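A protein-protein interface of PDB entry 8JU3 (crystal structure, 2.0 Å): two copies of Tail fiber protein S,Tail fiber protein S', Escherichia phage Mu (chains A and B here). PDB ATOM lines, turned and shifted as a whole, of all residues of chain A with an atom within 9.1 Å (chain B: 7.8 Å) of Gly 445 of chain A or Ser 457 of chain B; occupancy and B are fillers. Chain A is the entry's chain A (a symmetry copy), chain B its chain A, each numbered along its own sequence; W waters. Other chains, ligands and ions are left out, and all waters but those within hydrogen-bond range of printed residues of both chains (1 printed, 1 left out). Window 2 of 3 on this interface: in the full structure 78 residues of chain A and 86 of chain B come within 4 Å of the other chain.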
ATOM      1  N   SER A 437     -20.568 -19.537 -23.056  1.00  0.00           N
ATOM      2  CA  SER A 437     -20.196 -20.242 -21.839  1.00  0.00           C
ATOM      3  C   SER A 437     -19.651 -21.594 -22.230  1.00  0.00           C
ATOM      4  O   SER A 437     -19.811 -22.036 -23.371  1.00  0.00           O
ATOM      5  CB  SER A 437     -21.366 -20.417 -20.881  1.00  0.00           C
ATOM      6  OG  SER A 437     -22.502 -20.775 -21.626  1.00  0.00           O
ATOM      7  N   VAL A 438     -18.967 -22.214 -21.265  1.00  0.00           N
ATOM      8  CA  VAL A 438     -18.388 -23.537 -21.434  1.00  0.00           C
ATOM      9  C   VAL A 438     -18.472 -24.255 -20.096  1.00  0.00           C
ATOM     10  O   VAL A 438     -18.351 -23.641 -19.033  1.00  0.00           O
ATOM     11  CB  VAL A 438     -16.919 -23.474 -21.921  1.00  0.00           C
ATOM     12  CG1 VAL A 438     -16.850 -23.145 -23.416  1.00  0.00           C
ATOM     13  CG2 VAL A 438     -16.118 -22.497 -21.069  1.00  0.00           C
ATOM     14  N   GLN A 439     -18.676 -25.566 -20.147  1.00  0.00           N
ATOM     15  CA  GLN A 439     -18.633 -26.381 -18.941  1.00  0.00           C
ATOM     16  C   GLN A 439     -17.203 -26.863 -18.711  1.00  0.00           C
ATOM     17  O   GLN A 439     -16.494 -27.232 -19.653  1.00  0.00           O
ATOM     18  CB  GLN A 439     -19.604 -27.560 -19.052  1.00  0.00           C
ATOM     19  CG  GLN A 439     -19.126 -28.747 -19.900  1.00  0.00           C
ATOM     20  CD  GLN A 439     -18.867 -28.405 -21.370  1.00  0.00           C
ATOM     21  OE1 GLN A 439     -19.159 -27.289 -21.841  1.00  0.00           O
ATOM     22  NE2 GLN A 439     -18.326 -29.379 -22.107  1.00  0.00           N
ATOM     23  N   THR A 440     -16.768 -26.830 -17.456  1.00  0.00           N
ATOM     24  CA  THR A 440     -15.364 -27.100 -17.147  1.00  0.00           C
ATOM     25  C   THR A 440     -15.241 -28.330 -16.244  1.00  0.00           C
ATOM     26  O   THR A 440     -15.881 -29.357 -16.481  1.00  0.00           O
ATOM     27  CB  THR A 440     -14.685 -25.871 -16.471  1.00  0.00           C
ATOM     28  OG1 THR A 440     -15.084 -25.788 -15.097  1.00  0.00           O
ATOM     29  CG2 THR A 440     -15.104 -24.554 -17.186  1.00  0.00           C
ATOM     30  N   GLY A 445     -11.876 -25.576 -19.859  1.00  0.00           N
ATOM     31  CA  GLY A 445     -12.449 -24.297 -19.446  1.00  0.00           C
ATOM     32  C   GLY A 445     -12.543 -23.260 -20.560  1.00  0.00           C
ATOM     33  O   GLY A 445     -12.592 -23.609 -21.742  1.00  0.00           O
ATOM     34  N   TRP A 446     -12.589 -21.978 -20.209  1.00  0.00           N
ATOM     35  CA  TRP A 446     -12.606 -20.920 -21.217  1.00  0.00           C
ATOM     36  C   TRP A 446     -11.151 -20.507 -21.504  1.00  0.00           C
ATOM     37  O   TRP A 446     -10.451 -20.022 -20.609  1.00  0.00           O
ATOM     38  CB  TRP A 446     -13.461 -19.740 -20.756  1.00  0.00           C
ATOM     39  CG  TRP A 446     -13.492 -18.637 -21.811  1.00  0.00           C
ATOM     40  CD1 TRP A 446     -12.626 -17.603 -21.956  1.00  0.00           C
ATOM     41  CD2 TRP A 446     -14.442 -18.524 -22.876  1.00  0.00           C
ATOM     42  NE1 TRP A 446     -12.969 -16.854 -23.061  1.00  0.00           N
ATOM     43  CE2 TRP A 446     -14.072 -17.425 -23.649  1.00  0.00           C
ATOM     44  CE3 TRP A 446     -15.547 -19.297 -23.279  1.00  0.00           C
ATOM     45  CZ2 TRP A 446     -14.796 -17.029 -24.755  1.00  0.00           C
ATOM     46  CZ3 TRP A 446     -16.261 -18.904 -24.401  1.00  0.00           C
ATOM     47  CH2 TRP A 446     -15.873 -17.808 -25.126  1.00  0.00           C
ATOM     48  N   SER A 447     -10.687 -20.778 -22.728  1.00  0.00           N
ATOM     49  CA  SER A 447      -9.375 -20.356 -23.222  1.00  0.00           C
ATOM     50  C   SER A 447      -9.453 -18.939 -23.740  1.00  0.00           C
ATOM     51  O   SER A 447     -10.450 -18.548 -24.377  1.00  0.00           O
ATOM     52  CB  SER A 447      -8.896 -21.240 -24.397  1.00  0.00           C
ATOM     53  OG  SER A 447      -9.413 -22.514 -24.187  1.00  0.00           O
ATOM     54  N   ASP A 448      -8.369 -18.191 -23.504  1.00  0.00           N
ATOM     55  CA  ASP A 448      -8.249 -16.824 -23.979  1.00  0.00           C
ATOM     56  C   ASP A 448      -8.705 -16.742 -25.427  1.00  0.00           C
ATOM     57  O   ASP A 448      -8.301 -17.548 -26.272  1.00  0.00           O
ATOM     58  CB  ASP A 448      -6.796 -16.358 -23.823  1.00  0.00           C
ATOM     59  CG  ASP A 448      -6.567 -14.985 -24.401  1.00  0.00           C
ATOM     60  OD1 ASP A 448      -6.820 -13.943 -23.717  1.00  0.00           O
ATOM     61  OD2 ASP A 448      -6.180 -14.934 -25.597  1.00  0.00           O
ATOM     62  N   ARG A 449      -9.612 -15.820 -25.681  1.00  0.00           N
ATOM     63  CA  ARG A 449     -10.214 -15.574 -26.988  1.00  0.00           C
ATOM     64  C   ARG A 449     -10.221 -14.100 -27.304  1.00  0.00           C
ATOM     65  O   ARG A 449     -10.663 -13.276 -26.496  1.00  0.00           O
ATOM     66  CB  ARG A 449     -11.638 -16.155 -27.074  1.00  0.00           C
ATOM     67  CG  ARG A 449     -12.259 -16.201 -28.510  1.00  0.00           C
ATOM     68  CD  ARG A 449     -13.810 -16.544 -28.456  1.00  0.00           C
ATOM     69  NE  ARG A 449     -14.553 -16.234 -29.681  1.00  0.00           N
ATOM     70  CZ  ARG A 449     -15.816 -16.590 -29.937  1.00  0.00           C
ATOM     71  NH1 ARG A 449     -16.489 -17.437 -29.154  1.00  0.00           N
ATOM     72  NH2 ARG A 449     -16.428 -16.077 -31.003  1.00  0.00           N
ATOM     73  N   VAL A 453     -13.743 -11.437 -22.434  1.00  0.00           N
ATOM     74  CA  VAL A 453     -13.369 -11.376 -21.030  1.00  0.00           C
ATOM     75  C   VAL A 453     -14.296 -12.313 -20.278  1.00  0.00           C
ATOM     76  O   VAL A 453     -15.462 -12.477 -20.656  1.00  0.00           O
ATOM     77  CB  VAL A 453     -13.471  -9.934 -20.453  1.00  0.00           C
ATOM     78  CG1 VAL A 453     -12.489  -9.000 -21.233  1.00  0.00           C
ATOM     79  CG2 VAL A 453     -14.894  -9.340 -20.677  1.00  0.00           C
ATOM     80  N   VAL A 454     -13.774 -12.918 -19.216  1.00  0.00           N
ATOM     81  CA  VAL A 454     -14.582 -13.781 -18.351  1.00  0.00           C
ATOM     82  C   VAL A 454     -15.487 -12.889 -17.501  1.00  0.00           C
ATOM     83  O   VAL A 454     -15.062 -11.837 -16.980  1.00  0.00           O
ATOM     84  CB  VAL A 454     -13.676 -14.655 -17.487  1.00  0.00           C
ATOM     85  CG1 VAL A 454     -14.514 -15.458 -16.447  1.00  0.00           C
ATOM     86  CG2 VAL A 454     -12.761 -15.593 -18.377  1.00  0.00           C
ATOM     87  N   THR A 455     -16.763 -13.229 -17.461  1.00  0.00           N
ATOM     88  CA  THR A 455     -17.750 -12.467 -16.715  1.00  0.00           C
ATOM     89  C   THR A 455     -18.437 -13.323 -15.689  1.00  0.00           C
ATOM     90  O   THR A 455     -19.239 -12.794 -14.914  1.00  0.00           O
ATOM     91  CB  THR A 455     -18.824 -11.873 -17.658  1.00  0.00           C
ATOM     92  OG1 THR A 455     -19.564 -12.976 -18.277  1.00  0.00           O
ATOM     93  CG2 THR A 455     -18.160 -11.114 -18.722  1.00  0.00           C
ATOM     94  N   GLY A 456     -18.170 -14.620 -15.650  1.00  0.00           N
ATOM     95  CA  GLY A 456     -18.807 -15.416 -14.612  1.00  0.00           C
ATOM     96  C   GLY A 456     -18.131 -16.757 -14.474  1.00  0.00           C
ATOM     97  O   GLY A 456     -17.613 -17.302 -15.452  1.00  0.00           O
ATOM     98  N   SER A 457     -18.101 -17.283 -13.243  1.00  0.00           N
ATOM     99  CA  SER A 457     -17.589 -18.640 -12.965  1.00  0.00           C
ATOM    100  C   SER A 457     -18.634 -19.291 -12.070  1.00  0.00           C
ATOM    101  O   SER A 457     -18.437 -19.362 -10.857  1.00  0.00           O
ATOM    102  CB  SER A 457     -16.199 -18.635 -12.278  1.00  0.00           C
ATOM    103  OG  SER A 457     -15.173 -18.085 -13.076  1.00  0.00           O
ATOM    104  N   ASP A 467     -17.078 -25.952 -12.649  1.00  0.00           N
ATOM    105  CA  ASP A 467     -18.452 -25.847 -13.127  1.00  0.00           C
ATOM    106  C   ASP A 467     -18.498 -25.172 -14.518  1.00  0.00           C
ATOM    107  O   ASP A 467     -18.087 -25.769 -15.513  1.00  0.00           O
ATOM    108  CB  ASP A 467     -19.316 -25.064 -12.131  1.00  0.00           C
ATOM    109  CG  ASP A 467     -19.235 -25.620 -10.713  1.00  0.00           C
ATOM    110  OD1 ASP A 467     -18.460 -26.579 -10.490  1.00  0.00           O
ATOM    111  OD2 ASP A 467     -19.951 -25.096  -9.823  1.00  0.00           O
ATOM    112  N   THR A 468     -18.987 -23.934 -14.602  1.00  0.00           N
ATOM    113  CA  THR A 468     -19.151 -23.287 -15.897  1.00  0.00           C
ATOM    114  C   THR A 468     -18.518 -21.908 -15.894  1.00  0.00           C
ATOM    115  O   THR A 468     -18.577 -21.191 -14.890  1.00  0.00           O
ATOM    116  CB  THR A 468     -20.637 -23.204 -16.306  1.00  0.00           C
ATOM    117  OG1 THR A 468     -21.038 -24.460 -16.867  1.00  0.00           O
ATOM    118  CG2 THR A 468     -20.909 -22.046 -17.305  1.00  0.00           C
ATOM    119  N   THR A 469     -17.885 -21.559 -17.014  1.00  0.00           N
ATOM    120  CA  THR A 469     -17.280 -20.247 -17.187  1.00  0.00           C
ATOM    121  C   THR A 469     -18.031 -19.502 -18.298  1.00  0.00           C
ATOM    122  O   THR A 469     -18.333 -20.071 -19.352  1.00  0.00           O
ATOM    123  CB  THR A 469     -15.786 -20.365 -17.520  1.00  0.00           C
ATOM    124  OG1 THR A 469     -15.118 -21.124 -16.513  1.00  0.00           O
ATOM    125  CG2 THR A 469     -15.143 -18.990 -17.593  1.00  0.00           C
ATOM    126  N   GLN A 470     -18.349 -18.244 -18.032  1.00  0.00           N
ATOM    127  CA  GLN A 470     -19.026 -17.348 -18.944  1.00  0.00           C
ATOM    128  C   GLN A 470     -18.088 -16.220 -19.349  1.00  0.00           C
ATOM    129  O   GLN A 470     -17.328 -15.709 -18.516  1.00  0.00           O
ATOM    130  CB  GLN A 470     -20.265 -16.786 -18.262  1.00  0.00           C
ATOM    131  CG  GLN A 470     -21.022 -17.865 -17.422  1.00  0.00           C
ATOM    132  CD  GLN A 470     -22.120 -17.238 -16.588  1.00  0.00           C
ATOM    133  OE1 GLN A 470     -21.866 -16.700 -15.496  1.00  0.00           O
ATOM    134  NE2 GLN A 470     -23.351 -17.301 -17.091  1.00  0.00           N
ATOM    135  N   ALA A 471     -18.236 -15.781 -20.588  1.00  0.00           N
ATOM    136  CA  ALA A 471     -17.386 -14.788 -21.212  1.00  0.00           C
ATOM    137  C   ALA A 471     -18.238 -13.990 -22.169  1.00  0.00           C
ATOM    138  O   ALA A 471     -19.205 -14.520 -22.721  1.00  0.00           O
ATOM    139  CB  ALA A 471     -16.226 -15.510 -21.964  1.00  0.00           C
ATOM    140  N   THR B 440      -2.040 -21.918 -11.005  1.00  0.00           N
ATOM    141  CA  THR B 440      -2.803 -21.850  -9.760  1.00  0.00           C
ATOM    142  C   THR B 440      -2.852 -23.224  -9.084  1.00  0.00           C
ATOM    143  O   THR B 440      -1.836 -23.915  -8.981  1.00  0.00           O
ATOM    144  CB  THR B 440      -4.250 -21.327 -10.010  1.00  0.00           C
ATOM    145  OG1 THR B 440      -5.055 -22.370 -10.573  1.00  0.00           O
ATOM    146  CG2 THR B 440      -4.234 -20.127 -10.999  1.00  0.00           C
ATOM    147  N   VAL B 454      -9.546 -10.905 -16.292  1.00  0.00           N
ATOM    148  CA  VAL B 454      -9.302 -12.321 -16.573  1.00  0.00           C
ATOM    149  C   VAL B 454      -9.914 -12.649 -17.936  1.00  0.00           C
ATOM    150  O   VAL B 454     -11.037 -12.211 -18.266  1.00  0.00           O
ATOM    151  CB  VAL B 454      -9.892 -13.187 -15.465  1.00  0.00           C
ATOM    152  CG1 VAL B 454      -9.786 -14.698 -15.829  1.00  0.00           C
ATOM    153  CG2 VAL B 454      -9.232 -12.859 -14.062  1.00  0.00           C
ATOM    154  N   THR B 455      -9.138 -13.306 -18.778  1.00  0.00           N
ATOM    155  CA  THR B 455      -9.570 -13.669 -20.117  1.00  0.00           C
ATOM    156  C   THR B 455      -9.502 -15.155 -20.327  1.00  0.00           C
ATOM    157  O   THR B 455      -9.924 -15.626 -21.387  1.00  0.00           O
ATOM    158  CB  THR B 455      -8.696 -12.979 -21.191  1.00  0.00           C
ATOM    159  OG1 THR B 455      -7.326 -13.483 -21.070  1.00  0.00           O
ATOM    160  CG2 THR B 455      -8.676 -11.535 -20.938  1.00  0.00           C
ATOM    161  N   GLY B 456      -8.984 -15.916 -19.375  1.00  0.00           N
ATOM    162  CA  GLY B 456      -8.979 -17.357 -19.581  1.00  0.00           C
ATOM    163  C   GLY B 456      -8.706 -18.082 -18.288  1.00  0.00           C
ATOM    164  O   GLY B 456      -7.995 -17.572 -17.420  1.00  0.00           O
ATOM    165  N   SER B 457      -9.304 -19.271 -18.137  1.00  0.00           N
ATOM    166  CA  SER B 457      -9.042 -20.159 -16.987  1.00  0.00           C
ATOM    167  C   SER B 457      -8.812 -21.540 -17.586  1.00  0.00           C
ATOM    168  O   SER B 457      -9.718 -22.373 -17.557  1.00  0.00           O
ATOM    169  CB  SER B 457     -10.206 -20.187 -15.963  1.00  0.00           C
ATOM    170  OG  SER B 457     -10.440 -18.945 -15.336  1.00  0.00           O
ATOM    171  N   VAL B 458      -7.625 -21.757 -18.154  1.00  0.00           N
ATOM    172  CA  VAL B 458      -7.256 -23.044 -18.778  1.00  0.00           C
ATOM    173  C   VAL B 458      -7.773 -24.306 -18.048  1.00  0.00           C
ATOM    174  O   VAL B 458      -7.698 -24.432 -16.816  1.00  0.00           O
ATOM    175  CB  VAL B 458      -5.709 -23.123 -18.937  1.00  0.00           C
ATOM    176  CG1 VAL B 458      -5.271 -24.492 -19.444  1.00  0.00           C
ATOM    177  CG2 VAL B 458      -5.221 -22.020 -19.867  1.00  0.00           C
ATOM    178  N   ASP B 467      -5.697 -24.842 -12.437  1.00  0.00           N
ATOM    179  CA  ASP B 467      -4.743 -24.886 -13.540  1.00  0.00           C
ATOM    180  C   ASP B 467      -4.103 -23.496 -13.766  1.00  0.00           C
ATOM    181  O   ASP B 467      -3.299 -23.041 -12.952  1.00  0.00           O
ATOM    182  CB  ASP B 467      -5.422 -25.372 -14.826  1.00  0.00           C
ATOM    183  CG  ASP B 467      -6.160 -26.693 -14.644  1.00  0.00           C
ATOM    184  OD1 ASP B 467      -6.195 -27.205 -13.501  1.00  0.00           O
ATOM    185  OD2 ASP B 467      -6.701 -27.221 -15.648  1.00  0.00           O
ATOM    186  N   THR B 468      -4.450 -22.812 -14.857  1.00  0.00           N
ATOM    187  CA  THR B 468      -3.804 -21.546 -15.177  1.00  0.00           C
ATOM    188  C   THR B 468      -4.838 -20.470 -15.455  1.00  0.00           C
ATOM    189  O   THR B 468      -5.882 -20.741 -16.054  1.00  0.00           O
ATOM    190  CB  THR B 468      -2.833 -21.689 -16.367  1.00  0.00           C
ATOM    191  OG1 THR B 468      -1.588 -22.219 -15.893  1.00  0.00           O
ATOM    192  CG2 THR B 468      -2.607 -20.343 -17.108  1.00  0.00           C
ATOM    193  N   THR B 469      -4.550 -19.256 -14.984  1.00  0.00           N
ATOM    194  CA  THR B 469      -5.411 -18.108 -15.221  1.00  0.00           C
ATOM    195  C   THR B 469      -4.657 -17.100 -16.097  1.00  0.00           C
ATOM    196  O   THR B 469      -3.477 -16.817 -15.867  1.00  0.00           O
ATOM    197  CB  THR B 469      -5.853 -17.464 -13.900  1.00  0.00           C
ATOM    198  OG1 THR B 469      -6.486 -18.434 -13.068  1.00  0.00           O
ATOM    199  CG2 THR B 469      -6.835 -16.333 -14.156  1.00  0.00           C
ATOM    200  N   GLN B 470      -5.343 -16.594 -17.110  1.00  0.00           N
ATOM    201  CA  GLN B 470      -4.842 -15.605 -18.041  1.00  0.00           C
ATOM    202  C   GLN B 470      -5.609 -14.303 -17.870  1.00  0.00           C
ATOM    203  O   GLN B 470      -6.830 -14.318 -17.668  1.00  0.00           O
ATOM    204  CB  GLN B 470      -5.002 -16.131 -19.460  1.00  0.00           C
ATOM    205  CG  GLN B 470      -4.652 -17.651 -19.574  1.00  0.00           C
ATOM    206  CD  GLN B 470      -5.022 -18.197 -20.938  1.00  0.00           C
ATOM    207  OE1 GLN B 470      -6.188 -18.541 -21.194  1.00  0.00           O
ATOM    208  NE2 GLN B 470      -4.033 -18.283 -21.825  1.00  0.00           N
ATOM    209  N   ALA B 471      -4.901 -13.201 -18.066  1.00  0.00           N
ATOM    210  CA  ALA B 471      -5.403 -11.859 -17.859  1.00  0.00           C
ATOM    211  C   ALA B 471      -4.735 -10.957 -18.868  1.00  0.00           C
ATOM    212  O   ALA B 471      -3.597 -11.219 -19.269  1.00  0.00           O
ATOM    213  CB  ALA B 471      -5.072 -11.411 -16.402  1.00  0.00           C
HETATM  214  O   HOH W   1     -11.095 -14.713 -23.586  1.00  0.00           O
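Of the 19 printed residues of chain A, 5 touch a printed residue of chain B.
Of the 11 printed residues of chain B, 5 touch a printed residue of chain A.
Water W1 lies within hydrogen-bond range of the backbone carbonyl oxygen of Thr 455 of chain B (2.7 Å), the backbone NH of Arg 449 of chain A (2.8 Å) and the indole nitrogen of Trp 446 of chain A (2.9 Å).
Among the printed residues, pairs that only touch across the chains: Trp 446 of chain A with Gly 456 of chain B (3.2 Å), Trp 446 of chain A with Thr 455 of chain B (3.4 Å), Val 453 of chain A with Val 454 of chain B (3.7 Å), Val 454 of chain A with Thr 455 of chain B (3.8 Å), Gly 445 of chain A with Ser 457 of chain B (3.8 Å) and Val 454 of chain A with Gly 456 of chain B (3.9 Å).
The backbone carbonyl oxygen of Val 454 of chain B lies within hydrogen-bond range of the backbone NH of Val 454 of chain A (3.0 Å).
The side-chain hydroxyl of Thr 455 of chain B sits at hydrogen-bond distance from the side-chain carboxylate of Asp 448 of chain A (2.7 Å).
The backbone NH of Ser 457 of chain B sits at hydrogen-bond distance from the backbone carbonyl oxygen of Trp 446 of chain A (2.8 Å).
N of Asp 448 of chain A sits at hydrogen-bond distance from OE1 of Gln 470 of chain B, 3.2 Å away.
Val 454 of chain B touches its own counterpart, Val 454 of chain A.
Val 454 of chain A touches Thr 455 of chain B, but with the chains exchanged Thr 455 of chain A does not touch Val 454 of chain B (5.9 Å).
Val 454 of chain A touches Gly 456 of chain B, but with the chains exchanged Gly 456 of chain A does not touch Val 454 of chain B (8.0 Å).
The backbone NH (N) of Thr 455 of chain B lies within hydrogen-bond range of the backbone carbonyl oxygen (O) of Gln 470 of chain B.
O of Gly 456 of chain B is in hydrogen-bond range of N of Gln 470 of chain B (2.8 Å).
Gly 445 of chain A touches one residue of chain B.
Gly 456 of chain B touches just these residues of chain A: Trp 446 and Val 454.
No residue of chain A comes within 4 Å of Val 458 of chain B.
Printed residues of chain B within 4 Å of Asp 448 of chain A: Thr 455 (2.7 Å) and Gln 470 (3.2 Å).
Of the printed residues of chain B, Val 453 of chain A touches Val 454.
Thr 469 of chain A touches none of the printed residues of chain B.
Thr 455 of chain A touches none of the printed residues of chain B.
The nearest printed residue of chain A that does not touch Ser 457 of chain B is Ser 447 of chain A (5.0 Å).
The nearest printed residue of chain B that does not touch Val 454 of chain A is Ser 457 of chain B (5.1 Å).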
